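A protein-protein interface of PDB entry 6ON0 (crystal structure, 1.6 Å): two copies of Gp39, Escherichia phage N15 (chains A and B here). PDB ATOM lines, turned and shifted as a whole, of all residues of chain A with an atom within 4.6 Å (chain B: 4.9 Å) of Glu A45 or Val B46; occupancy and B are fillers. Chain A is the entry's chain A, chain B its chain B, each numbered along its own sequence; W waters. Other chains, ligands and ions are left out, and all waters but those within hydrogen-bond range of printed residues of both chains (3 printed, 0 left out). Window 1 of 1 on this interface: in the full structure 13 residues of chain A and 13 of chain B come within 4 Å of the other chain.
OG of Ser A42 sits at hydrogen-bond distance from OD1 of Asp B43.
OH of Tyr B50 sits at hydrogen-bond distance from OE2 of Glu A45, 2.5 Å away.
OH of Tyr A50 lies close to OE2 of Glu B45, 2.4 Å away.
OD1 of Asp A43 is in hydrogen-bond range of OG of Ser B42 (2.6 Å).
O of Glu B45 sits at hydrogen-bond distance from OG1 of Thr B48, at 3.4 Å.
The backbone carbonyl oxygen (O) of Glu B45 is in hydrogen-bond range of the backbone NH (N) of Tyr B50 (2.7 Å).
The backbone carbonyl oxygen (O) of Glu A45 is in hydrogen-bond range of the side-chain hydroxyl (OG1) of Thr A48 (3.3 Å).
The side-chain hydroxyl (OG) of Ser A54 sits close to the backbone NH (N) of Phe A56, 3.4 Å away.
The side-chain carboxylate (OD1) of Asp B43 lies within salt-bridge range of the guanidinium group (NE) of Arg B47 (3.0 Å).
OG of Ser A54 sits at hydrogen-bond distance from N of Thr A57, at 3.0 Å.
Among the printed residues, pairs that only touch across the chains: Thr A57 with Tyr B50 (3.4 Å), Phe A56 with Arg B47 (3.5 Å), Thr A57 with Val B46 (3.5 Å), Ser A54 with Val B46 (3.6 Å), Ser A42 with Val B46 (3.6 Å), Tyr A50 with Tyr B50 (3.6 Å), Val A46 with Glu B45 (3.6 Å), Phe A56 with Val B46 (3.7 Å), Val A46 with Ser B42 (3.7 Å), Glu A45 with Val B46 (3.8 Å) and Ser A42 with Ser B42 (3.9 Å).
Of the printed residues of chain B, Asp A43 touches Ser B42.
Glu A45 touches just these residues of chain B: Val B46 (3.8 Å) and Tyr B50 (2.5 Å).
Arg A47 touches none of the printed residues of chain B.
Leu A52 touches none of the printed residues of chain B.
Of the printed residues of chain A, Ser B42 touches Ser A42, Asp A43 and Val A46.
Of the printed residues of chain A, Val B46 touches Ser A42 (3.6 Å), Glu A45 (3.8 Å), Ser A54 (3.6 Å), Phe A56 (3.7 Å) and Thr A57 (3.5 Å).
The nearest printed residue of chain B that does not touch Glu A45 is Glu B45 (6.6 Å).
Of the 9 printed residues of chain B, 6 touch a printed residue of chain A.
Hydrophobic or aromatic side chains of chain B within 4 Å of the printed part of chain A: Val B46 and Tyr B50.
Of the 17 printed residues of chain A, 8 touch a printed residue of chain B.
Ser A42 touches Asp B43, and with the chains exchanged Asp A43 touches Ser B42.
Glu A45 touches Val B46, and with the chains exchanged Val A46 touches Glu B45.
Glu A45 touches Tyr B50, and with the chains exchanged Tyr A50 touches Glu B45.
Tyr A50 touches its own counterpart, Tyr B50.
9 positions are printed for both chains.
Of the 15 pairs that touch across the chains among the printed residues, 10 have their exchanged pair printed and touching as well.
Water W3 lies within hydrogen-bond range of OG1 of Thr A57 (2.7 Å) and O of Val B46 (2.7 Å).
Water W2 lies within hydrogen-bond range of OG of Ser A42 (2.8 Å) and NH2 of Arg B47 (2.9 Å).
Water W1 lies within hydrogen-bond range of the side-chain hydroxyl of Ser B42 and the guanidinium group of Arg A47.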
ATOM      1  N   MET A   1      10.034 -21.515  19.710  1.00  0.00           N
ATOM      2  CA  MET A   1       9.748 -22.388  18.561  1.00  0.00           C
ATOM      3  C   MET A   1      11.056 -23.059  18.115  1.00  0.00           C
ATOM      4  O   MET A   1      12.114 -22.441  18.273  1.00  0.00           O
ATOM      5  CB  MET A   1       9.129 -21.622  17.377  1.00  0.00           C
ATOM      6  CG  MET A   1      10.130 -20.847  16.478  1.00  0.00           C
ATOM      7  SD  MET A   1      10.805 -19.380  17.348  1.00  0.00           S
ATOM      8  CE  MET A   1       9.353 -18.353  17.593  1.00  0.00           C
ATOM      9  N   GLN A  41      14.362 -15.861  18.815  1.00  0.00           N
ATOM     10  CA  GLN A  41      13.026 -16.473  19.051  1.00  0.00           C
ATOM     11  C   GLN A  41      12.004 -15.355  19.343  1.00  0.00           C
ATOM     12  O   GLN A  41      10.916 -15.371  18.769  1.00  0.00           O
ATOM     13  CB  GLN A  41      13.084 -17.514  20.164  1.00  0.00           C
ATOM     14  CG  GLN A  41      13.734 -18.828  19.739  1.00  0.00           C
ATOM     15  CD  GLN A  41      13.338 -19.948  20.661  1.00  0.00           C
ATOM     16  OE1 GLN A  41      12.162 -20.063  21.022  1.00  0.00           O
ATOM     17  NE2 GLN A  41      14.309 -20.792  21.024  1.00  0.00           N
ATOM     18  N   SER A  42      12.347 -14.387  20.188  1.00  0.00           N
ATOM     19  CA  SER A  42      11.463 -13.258  20.536  1.00  0.00           C
ATOM     20  C   SER A  42      11.143 -12.443  19.281  1.00  0.00           C
ATOM     21  O   SER A  42       9.934 -12.208  19.016  1.00  0.00           O
ATOM     22  CB  SER A  42      12.080 -12.448  21.641  1.00  0.00           C
ATOM     23  OG  SER A  42      12.052 -13.162  22.890  1.00  0.00           O
ATOM     24  N   ASP A  43      12.174 -12.141  18.476  1.00  0.00           N
ATOM     25  CA  ASP A  43      12.010 -11.343  17.235  1.00  0.00           C
ATOM     26  C   ASP A  43      11.097 -12.079  16.236  1.00  0.00           C
ATOM     27  O   ASP A  43      10.238 -11.415  15.627  1.00  0.00           O
ATOM     28  CB  ASP A  43      13.352 -10.929  16.665  1.00  0.00           C
ATOM     29  CG  ASP A  43      13.267  -9.756  15.726  1.00  0.00           C
ATOM     30  OD1 ASP A  43      12.734  -8.649  16.150  1.00  0.00           O
ATOM     31  OD2 ASP A  43      13.594  -9.988  14.521  1.00  0.00           O
ATOM     32  N   ILE A  44      11.247 -13.385  16.092  1.00  0.00           N
ATOM     33  CA  ILE A  44      10.421 -14.186  15.145  1.00  0.00           C
ATOM     34  C   ILE A  44       8.959 -14.164  15.624  1.00  0.00           C
ATOM     35  O   ILE A  44       8.049 -13.946  14.797  1.00  0.00           O
ATOM     36  CB  ILE A  44      10.962 -15.623  15.032  1.00  0.00           C
ATOM     37  CG1 ILE A  44      12.348 -15.644  14.393  1.00  0.00           C
ATOM     38  CG2 ILE A  44       9.975 -16.455  14.243  1.00  0.00           C
ATOM     39  CD1 ILE A  44      13.013 -16.989  14.443  1.00  0.00           C
ATOM     40  N   GLU A  45       8.763 -14.299  16.933  1.00  0.00           N
ATOM     41  CA  GLU A  45       7.419 -14.222  17.530  1.00  0.00           C
ATOM     42  C   GLU A  45       6.775 -12.876  17.184  1.00  0.00           C
ATOM     43  O   GLU A  45       5.628 -12.864  16.705  1.00  0.00           O
ATOM     44  CB  GLU A  45       7.487 -14.487  19.025  1.00  0.00           C
ATOM     45  CG  GLU A  45       6.149 -14.353  19.705  1.00  0.00           C
ATOM     46  CD  GLU A  45       6.184 -14.770  21.167  1.00  0.00           C
ATOM     47  OE1 GLU A  45       7.094 -15.517  21.535  1.00  0.00           O
ATOM     48  OE2 GLU A  45       5.320 -14.339  21.922  1.00  0.00           O
ATOM     49  N   VAL A  46       7.471 -11.780  17.412  1.00  0.00           N
ATOM     50  CA  VAL A  46       6.934 -10.415  17.161  1.00  0.00           C
ATOM     51  C   VAL A  46       6.702 -10.237  15.647  1.00  0.00           C
ATOM     52  O   VAL A  46       5.640  -9.761  15.259  1.00  0.00           O
ATOM     53  CB  VAL A  46       7.915  -9.404  17.762  1.00  0.00           C
ATOM     54  CG1 VAL A  46       7.742  -7.998  17.215  1.00  0.00           C
ATOM     55  CG2 VAL A  46       7.793  -9.468  19.300  1.00  0.00           C
ATOM     56  N   ARG A  47       7.673 -10.665  14.831  1.00  0.00           N
ATOM     57  CA  ARG A  47       7.642 -10.376  13.375  1.00  0.00           C
ATOM     58  C   ARG A  47       6.591 -11.243  12.692  1.00  0.00           C
ATOM     59  O   ARG A  47       6.190 -10.864  11.560  1.00  0.00           O
ATOM     60  CB  ARG A  47       9.039 -10.504  12.781  1.00  0.00           C
ATOM     61  CG  ARG A  47       9.793  -9.197  13.007  1.00  0.00           C
ATOM     62  CD  ARG A  47      11.305  -9.197  13.066  1.00  0.00           C
ATOM     63  NE  ARG A  47      11.730  -7.931  12.510  1.00  0.00           N
ATOM     64  CZ  ARG A  47      11.796  -6.732  13.084  1.00  0.00           C
ATOM     65  NH1 ARG A  47      11.578  -6.542  14.365  1.00  0.00           N
ATOM     66  NH2 ARG A  47      12.128  -5.702  12.333  1.00  0.00           N
ATOM     67  N   THR A  48       6.176 -12.348  13.306  1.00  0.00           N
ATOM     68  CA  THR A  48       5.111 -13.215  12.739  1.00  0.00           C
ATOM     69  C   THR A  48       3.764 -12.836  13.365  1.00  0.00           C
ATOM     70  O   THR A  48       2.820 -13.585  13.164  1.00  0.00           O
ATOM     71  CB  THR A  48       5.419 -14.706  12.894  1.00  0.00           C
ATOM     72  OG1 THR A  48       5.560 -15.081  14.260  1.00  0.00           O
ATOM     73  CG2 THR A  48       6.634 -15.066  12.079  1.00  0.00           C
ATOM     74  N   ALA A  49       3.663 -11.699  14.062  1.00  0.00           N
ATOM     75  CA  ALA A  49       2.394 -11.282  14.720  1.00  0.00           C
ATOM     76  C   ALA A  49       1.914 -12.426  15.630  1.00  0.00           C
ATOM     77  O   ALA A  49       0.693 -12.704  15.656  1.00  0.00           O
ATOM     78  CB  ALA A  49       1.334 -10.924  13.699  1.00  0.00           C
ATOM     79  N   TYR A  50       2.863 -13.080  16.316  1.00  0.00           N
ATOM     80  CA  TYR A  50       2.628 -14.123  17.351  1.00  0.00           C
ATOM     81  C   TYR A  50       2.145 -15.448  16.736  1.00  0.00           C
ATOM     82  O   TYR A  50       1.728 -16.328  17.499  1.00  0.00           O
ATOM     83  CB  TYR A  50       1.653 -13.588  18.420  1.00  0.00           C
ATOM     84  CG  TYR A  50       1.899 -12.156  18.822  1.00  0.00           C
ATOM     85  CD1 TYR A  50       3.124 -11.769  19.337  1.00  0.00           C
ATOM     86  CD2 TYR A  50       0.930 -11.172  18.670  1.00  0.00           C
ATOM     87  CE1 TYR A  50       3.385 -10.464  19.722  1.00  0.00           C
ATOM     88  CE2 TYR A  50       1.190  -9.846  19.010  1.00  0.00           C
ATOM     89  CZ  TYR A  50       2.418  -9.496  19.554  1.00  0.00           C
ATOM     90  OH  TYR A  50       2.673  -8.210  19.935  1.00  0.00           O
ATOM     91  N   LYS A  51       2.216 -15.617  15.416  1.00  0.00           N
ATOM     92  CA  LYS A  51       1.861 -16.892  14.745  1.00  0.00           C
ATOM     93  C   LYS A  51       2.869 -17.975  15.166  1.00  0.00           C
ATOM     94  O   LYS A  51       2.442 -19.085  15.346  1.00  0.00           O
ATOM     95  CB  LYS A  51       1.685 -16.616  13.247  1.00  0.00           C
ATOM     96  CG  LYS A  51       0.406 -15.816  12.974  1.00  0.00           C
ATOM     97  CD  LYS A  51       0.152 -15.460  11.513  1.00  0.00           C
ATOM     98  CE  LYS A  51       1.256 -14.592  10.914  1.00  0.00           C
ATOM     99  NZ  LYS A  51       0.840 -14.170   9.553  1.00  0.00           N
ATOM    100  N   LEU A  52       4.153 -17.657  15.372  1.00  0.00           N
ATOM    101  CA  LEU A  52       5.135 -18.591  15.978  1.00  0.00           C
ATOM    102  C   LEU A  52       5.445 -18.075  17.368  1.00  0.00           C
ATOM    103  O   LEU A  52       5.641 -16.853  17.500  1.00  0.00           O
ATOM    104  CB  LEU A  52       6.429 -18.618  15.167  1.00  0.00           C
ATOM    105  CG  LEU A  52       6.304 -19.127  13.742  1.00  0.00           C
ATOM    106  CD1 LEU A  52       7.662 -19.104  13.077  1.00  0.00           C
ATOM    107  CD2 LEU A  52       5.754 -20.556  13.742  1.00  0.00           C
ATOM    108  N   LYS A  53       5.485 -18.975  18.329  1.00  0.00           N
ATOM    109  CA  LYS A  53       5.741 -18.664  19.752  1.00  0.00           C
ATOM    110  C   LYS A  53       7.186 -19.035  20.086  1.00  0.00           C
ATOM    111  O   LYS A  53       7.575 -20.171  19.811  1.00  0.00           O
ATOM    112  CB  LYS A  53       4.832 -19.503  20.639  1.00  0.00           C
ATOM    113  CG  LYS A  53       3.367 -19.476  20.254  1.00  0.00           C
ATOM    114  CD  LYS A  53       2.806 -18.113  20.209  1.00  0.00           C
ATOM    115  CE  LYS A  53       1.310 -18.204  20.442  1.00  0.00           C
ATOM    116  NZ  LYS A  53       0.636 -16.971  19.984  1.00  0.00           N
ATOM    117  N   SER A  54       7.917 -18.095  20.698  1.00  0.00           N
ATOM    118  CA  SER A  54       9.165 -18.375  21.435  1.00  0.00           C
ATOM    119  C   SER A  54       8.912 -19.495  22.464  1.00  0.00           C
ATOM    120  O   SER A  54       7.777 -19.703  22.965  1.00  0.00           O
ATOM    121  CB  SER A  54       9.666 -17.111  22.079  1.00  0.00           C
ATOM    122  OG  SER A  54       8.833 -16.793  23.193  1.00  0.00           O
ATOM    123  N   PHE A  56       9.987 -19.165  25.411  1.00  0.00           N
ATOM    124  CA  PHE A  56       9.559 -18.389  26.602  1.00  0.00           C
ATOM    125  C   PHE A  56       8.011 -18.306  26.654  1.00  0.00           C
ATOM    126  O   PHE A  56       7.383 -18.645  27.696  1.00  0.00           O
ATOM    127  CB  PHE A  56      10.177 -16.994  26.605  1.00  0.00           C
ATOM    128  CG  PHE A  56       9.786 -16.177  27.820  1.00  0.00           C
ATOM    129  CD1 PHE A  56      10.578 -16.181  28.955  1.00  0.00           C
ATOM    130  CD2 PHE A  56       8.617 -15.438  27.824  1.00  0.00           C
ATOM    131  CE1 PHE A  56      10.220 -15.445  30.072  1.00  0.00           C
ATOM    132  CE2 PHE A  56       8.267 -14.688  28.932  1.00  0.00           C
ATOM    133  CZ  PHE A  56       9.052 -14.717  30.065  1.00  0.00           C
ATOM    134  N   THR A  57       7.376 -17.902  25.550  1.00  0.00           N
ATOM    135  CA  THR A  57       5.902 -17.722  25.496  1.00  0.00           C
ATOM    136  C   THR A  57       5.208 -19.086  25.678  1.00  0.00           C
ATOM    137  O   THR A  57       4.257 -19.169  26.486  1.00  0.00           O
ATOM    138  CB  THR A  57       5.495 -16.978  24.216  1.00  0.00           C
ATOM    139  OG1 THR A  57       6.085 -15.680  24.273  1.00  0.00           O
ATOM    140  CG2 THR A  57       3.986 -16.882  24.057  1.00  0.00           C
ATOM    141  N   SER B  42      11.908  -6.591  20.821  1.00  0.00           N
ATOM    142  CA  SER B  42      11.129  -7.844  20.643  1.00  0.00           C
ATOM    143  C   SER B  42      11.230  -8.677  21.909  1.00  0.00           C
ATOM    144  O   SER B  42      10.235  -9.129  22.400  1.00  0.00           O
ATOM    145  CB  SER B  42      11.633  -8.624  19.426  1.00  0.00           C
ATOM    146  OG  SER B  42      11.321  -7.938  18.235  1.00  0.00           O
ATOM    147  N   ASP B  43      12.420  -8.834  22.450  1.00  0.00           N
ATOM    148  CA  ASP B  43      12.608  -9.650  23.666  1.00  0.00           C
ATOM    149  C   ASP B  43      11.885  -9.046  24.867  1.00  0.00           C
ATOM    150  O   ASP B  43      11.288  -9.816  25.667  1.00  0.00           O
ATOM    151  CB  ASP B  43      14.083  -9.814  23.968  1.00  0.00           C
ATOM    152  CG  ASP B  43      14.274 -10.972  24.894  1.00  0.00           C
ATOM    153  OD1 ASP B  43      13.809 -12.078  24.545  1.00  0.00           O
ATOM    154  OD2 ASP B  43      14.856 -10.724  25.945  1.00  0.00           O
ATOM    155  N   ILE B  44      11.904  -7.731  24.992  1.00  0.00           N
ATOM    156  CA  ILE B  44      11.176  -7.050  26.091  1.00  0.00           C
ATOM    157  C   ILE B  44       9.667  -7.254  25.919  1.00  0.00           C
ATOM    158  O   ILE B  44       8.942  -7.601  26.925  1.00  0.00           O
ATOM    159  CB  ILE B  44      11.586  -5.574  26.190  1.00  0.00           C
ATOM    160  CG1 ILE B  44      13.071  -5.432  26.556  1.00  0.00           C
ATOM    161  CG2 ILE B  44      10.693  -4.905  27.222  1.00  0.00           C
ATOM    162  CD1 ILE B  44      13.583  -4.025  26.472  1.00  0.00           C
ATOM    163  N   GLU B  45       9.192  -7.097  24.697  1.00  0.00           N
ATOM    164  CA  GLU B  45       7.749  -7.275  24.404  1.00  0.00           C
ATOM    165  C   GLU B  45       7.360  -8.708  24.811  1.00  0.00           C
ATOM    166  O   GLU B  45       6.386  -8.878  25.535  1.00  0.00           O
ATOM    167  CB  GLU B  45       7.494  -6.942  22.933  1.00  0.00           C
ATOM    168  CG  GLU B  45       6.176  -7.471  22.425  1.00  0.00           C
ATOM    169  CD  GLU B  45       5.790  -6.968  21.031  1.00  0.00           C
ATOM    170  OE1 GLU B  45       6.475  -6.068  20.510  1.00  0.00           O
ATOM    171  OE2 GLU B  45       4.825  -7.436  20.491  1.00  0.00           O
ATOM    172  N   VAL B  46       8.151  -9.705  24.406  1.00  0.00           N
ATOM    173  CA  VAL B  46       7.891 -11.138  24.759  1.00  0.00           C
ATOM    174  C   VAL B  46       7.981 -11.329  26.295  1.00  0.00           C
ATOM    175  O   VAL B  46       7.024 -11.872  26.885  1.00  0.00           O
ATOM    176  CB  VAL B  46       8.833 -12.078  23.969  1.00  0.00           C
ATOM    177  CG1 VAL B  46       8.785 -13.486  24.513  1.00  0.00           C
ATOM    178  CG2 VAL B  46       8.496 -12.078  22.488  1.00  0.00           C
ATOM    179  N   ARG B  47       9.072 -10.876  26.918  1.00  0.00           N
ATOM    180  CA  ARG B  47       9.370 -11.210  28.346  1.00  0.00           C
ATOM    181  C   ARG B  47       8.353 -10.496  29.245  1.00  0.00           C
ATOM    182  O   ARG B  47       8.135 -11.001  30.336  1.00  0.00           O
ATOM    183  CB  ARG B  47      10.851 -10.966  28.685  1.00  0.00           C
ATOM    184  CG  ARG B  47      11.714 -12.072  28.086  1.00  0.00           C
ATOM    185  CD  ARG B  47      13.198 -12.234  28.427  1.00  0.00           C
ATOM    186  NE  ARG B  47      13.589 -13.158  27.357  1.00  0.00           N
ATOM    187  CZ  ARG B  47      13.826 -14.472  27.443  1.00  0.00           C
ATOM    188  NH1 ARG B  47      13.864 -15.101  28.615  1.00  0.00           N
ATOM    189  NH2 ARG B  47      14.117 -15.131  26.327  1.00  0.00           N
ATOM    190  N   THR B  48       7.735  -9.390  28.800  1.00  0.00           N
ATOM    191  CA  THR B  48       6.675  -8.664  29.578  1.00  0.00           C
ATOM    192  C   THR B  48       5.264  -9.115  29.176  1.00  0.00           C
ATOM    193  O   THR B  48       4.291  -8.453  29.609  1.00  0.00           O
ATOM    194  CB  THR B  48       6.756  -7.143  29.439  1.00  0.00           C
ATOM    195  OG1 THR B  48       6.551  -6.715  28.091  1.00  0.00           O
ATOM    196  CG2 THR B  48       8.067  -6.615  29.951  1.00  0.00           C
ATOM    197  N   ALA B  49       5.143 -10.208  28.407  1.00  0.00           N
ATOM    198  CA  ALA B  49       3.853 -10.738  27.913  1.00  0.00           C
ATOM    199  C   ALA B  49       3.118  -9.622  27.183  1.00  0.00           C
ATOM    200  O   ALA B  49       1.892  -9.481  27.360  1.00  0.00           O
ATOM    201  CB  ALA B  49       3.040 -11.289  29.061  1.00  0.00           C
ATOM    202  N   TYR B  50       3.841  -8.871  26.366  1.00  0.00           N
ATOM    203  CA  TYR B  50       3.317  -7.803  25.478  1.00  0.00           C
ATOM    204  C   TYR B  50       2.756  -6.631  26.277  1.00  0.00           C
ATOM    205  O   TYR B  50       2.081  -5.799  25.662  1.00  0.00           O
ATOM    206  CB  TYR B  50       2.220  -8.334  24.549  1.00  0.00           C
ATOM    207  CG  TYR B  50       2.433  -9.764  24.136  1.00  0.00           C
ATOM    208  CD1 TYR B  50       3.613 -10.145  23.508  1.00  0.00           C
ATOM    209  CD2 TYR B  50       1.510 -10.752  24.457  1.00  0.00           C
ATOM    210  CE1 TYR B  50       3.856 -11.452  23.149  1.00  0.00           C
ATOM    211  CE2 TYR B  50       1.745 -12.078  24.118  1.00  0.00           C
ATOM    212  CZ  TYR B  50       2.913 -12.415  23.435  1.00  0.00           C
ATOM    213  OH  TYR B  50       3.155 -13.700  23.054  1.00  0.00           O
HETATM  214  O   HOH W   1      11.736  -5.269  17.318  1.00  0.00           O
HETATM  215  O   HOH W   2      12.962 -15.713  23.684  1.00  0.00           O
HETATM  216  O   HOH W   3       5.435 -14.047  26.363  1.00  0.00           O
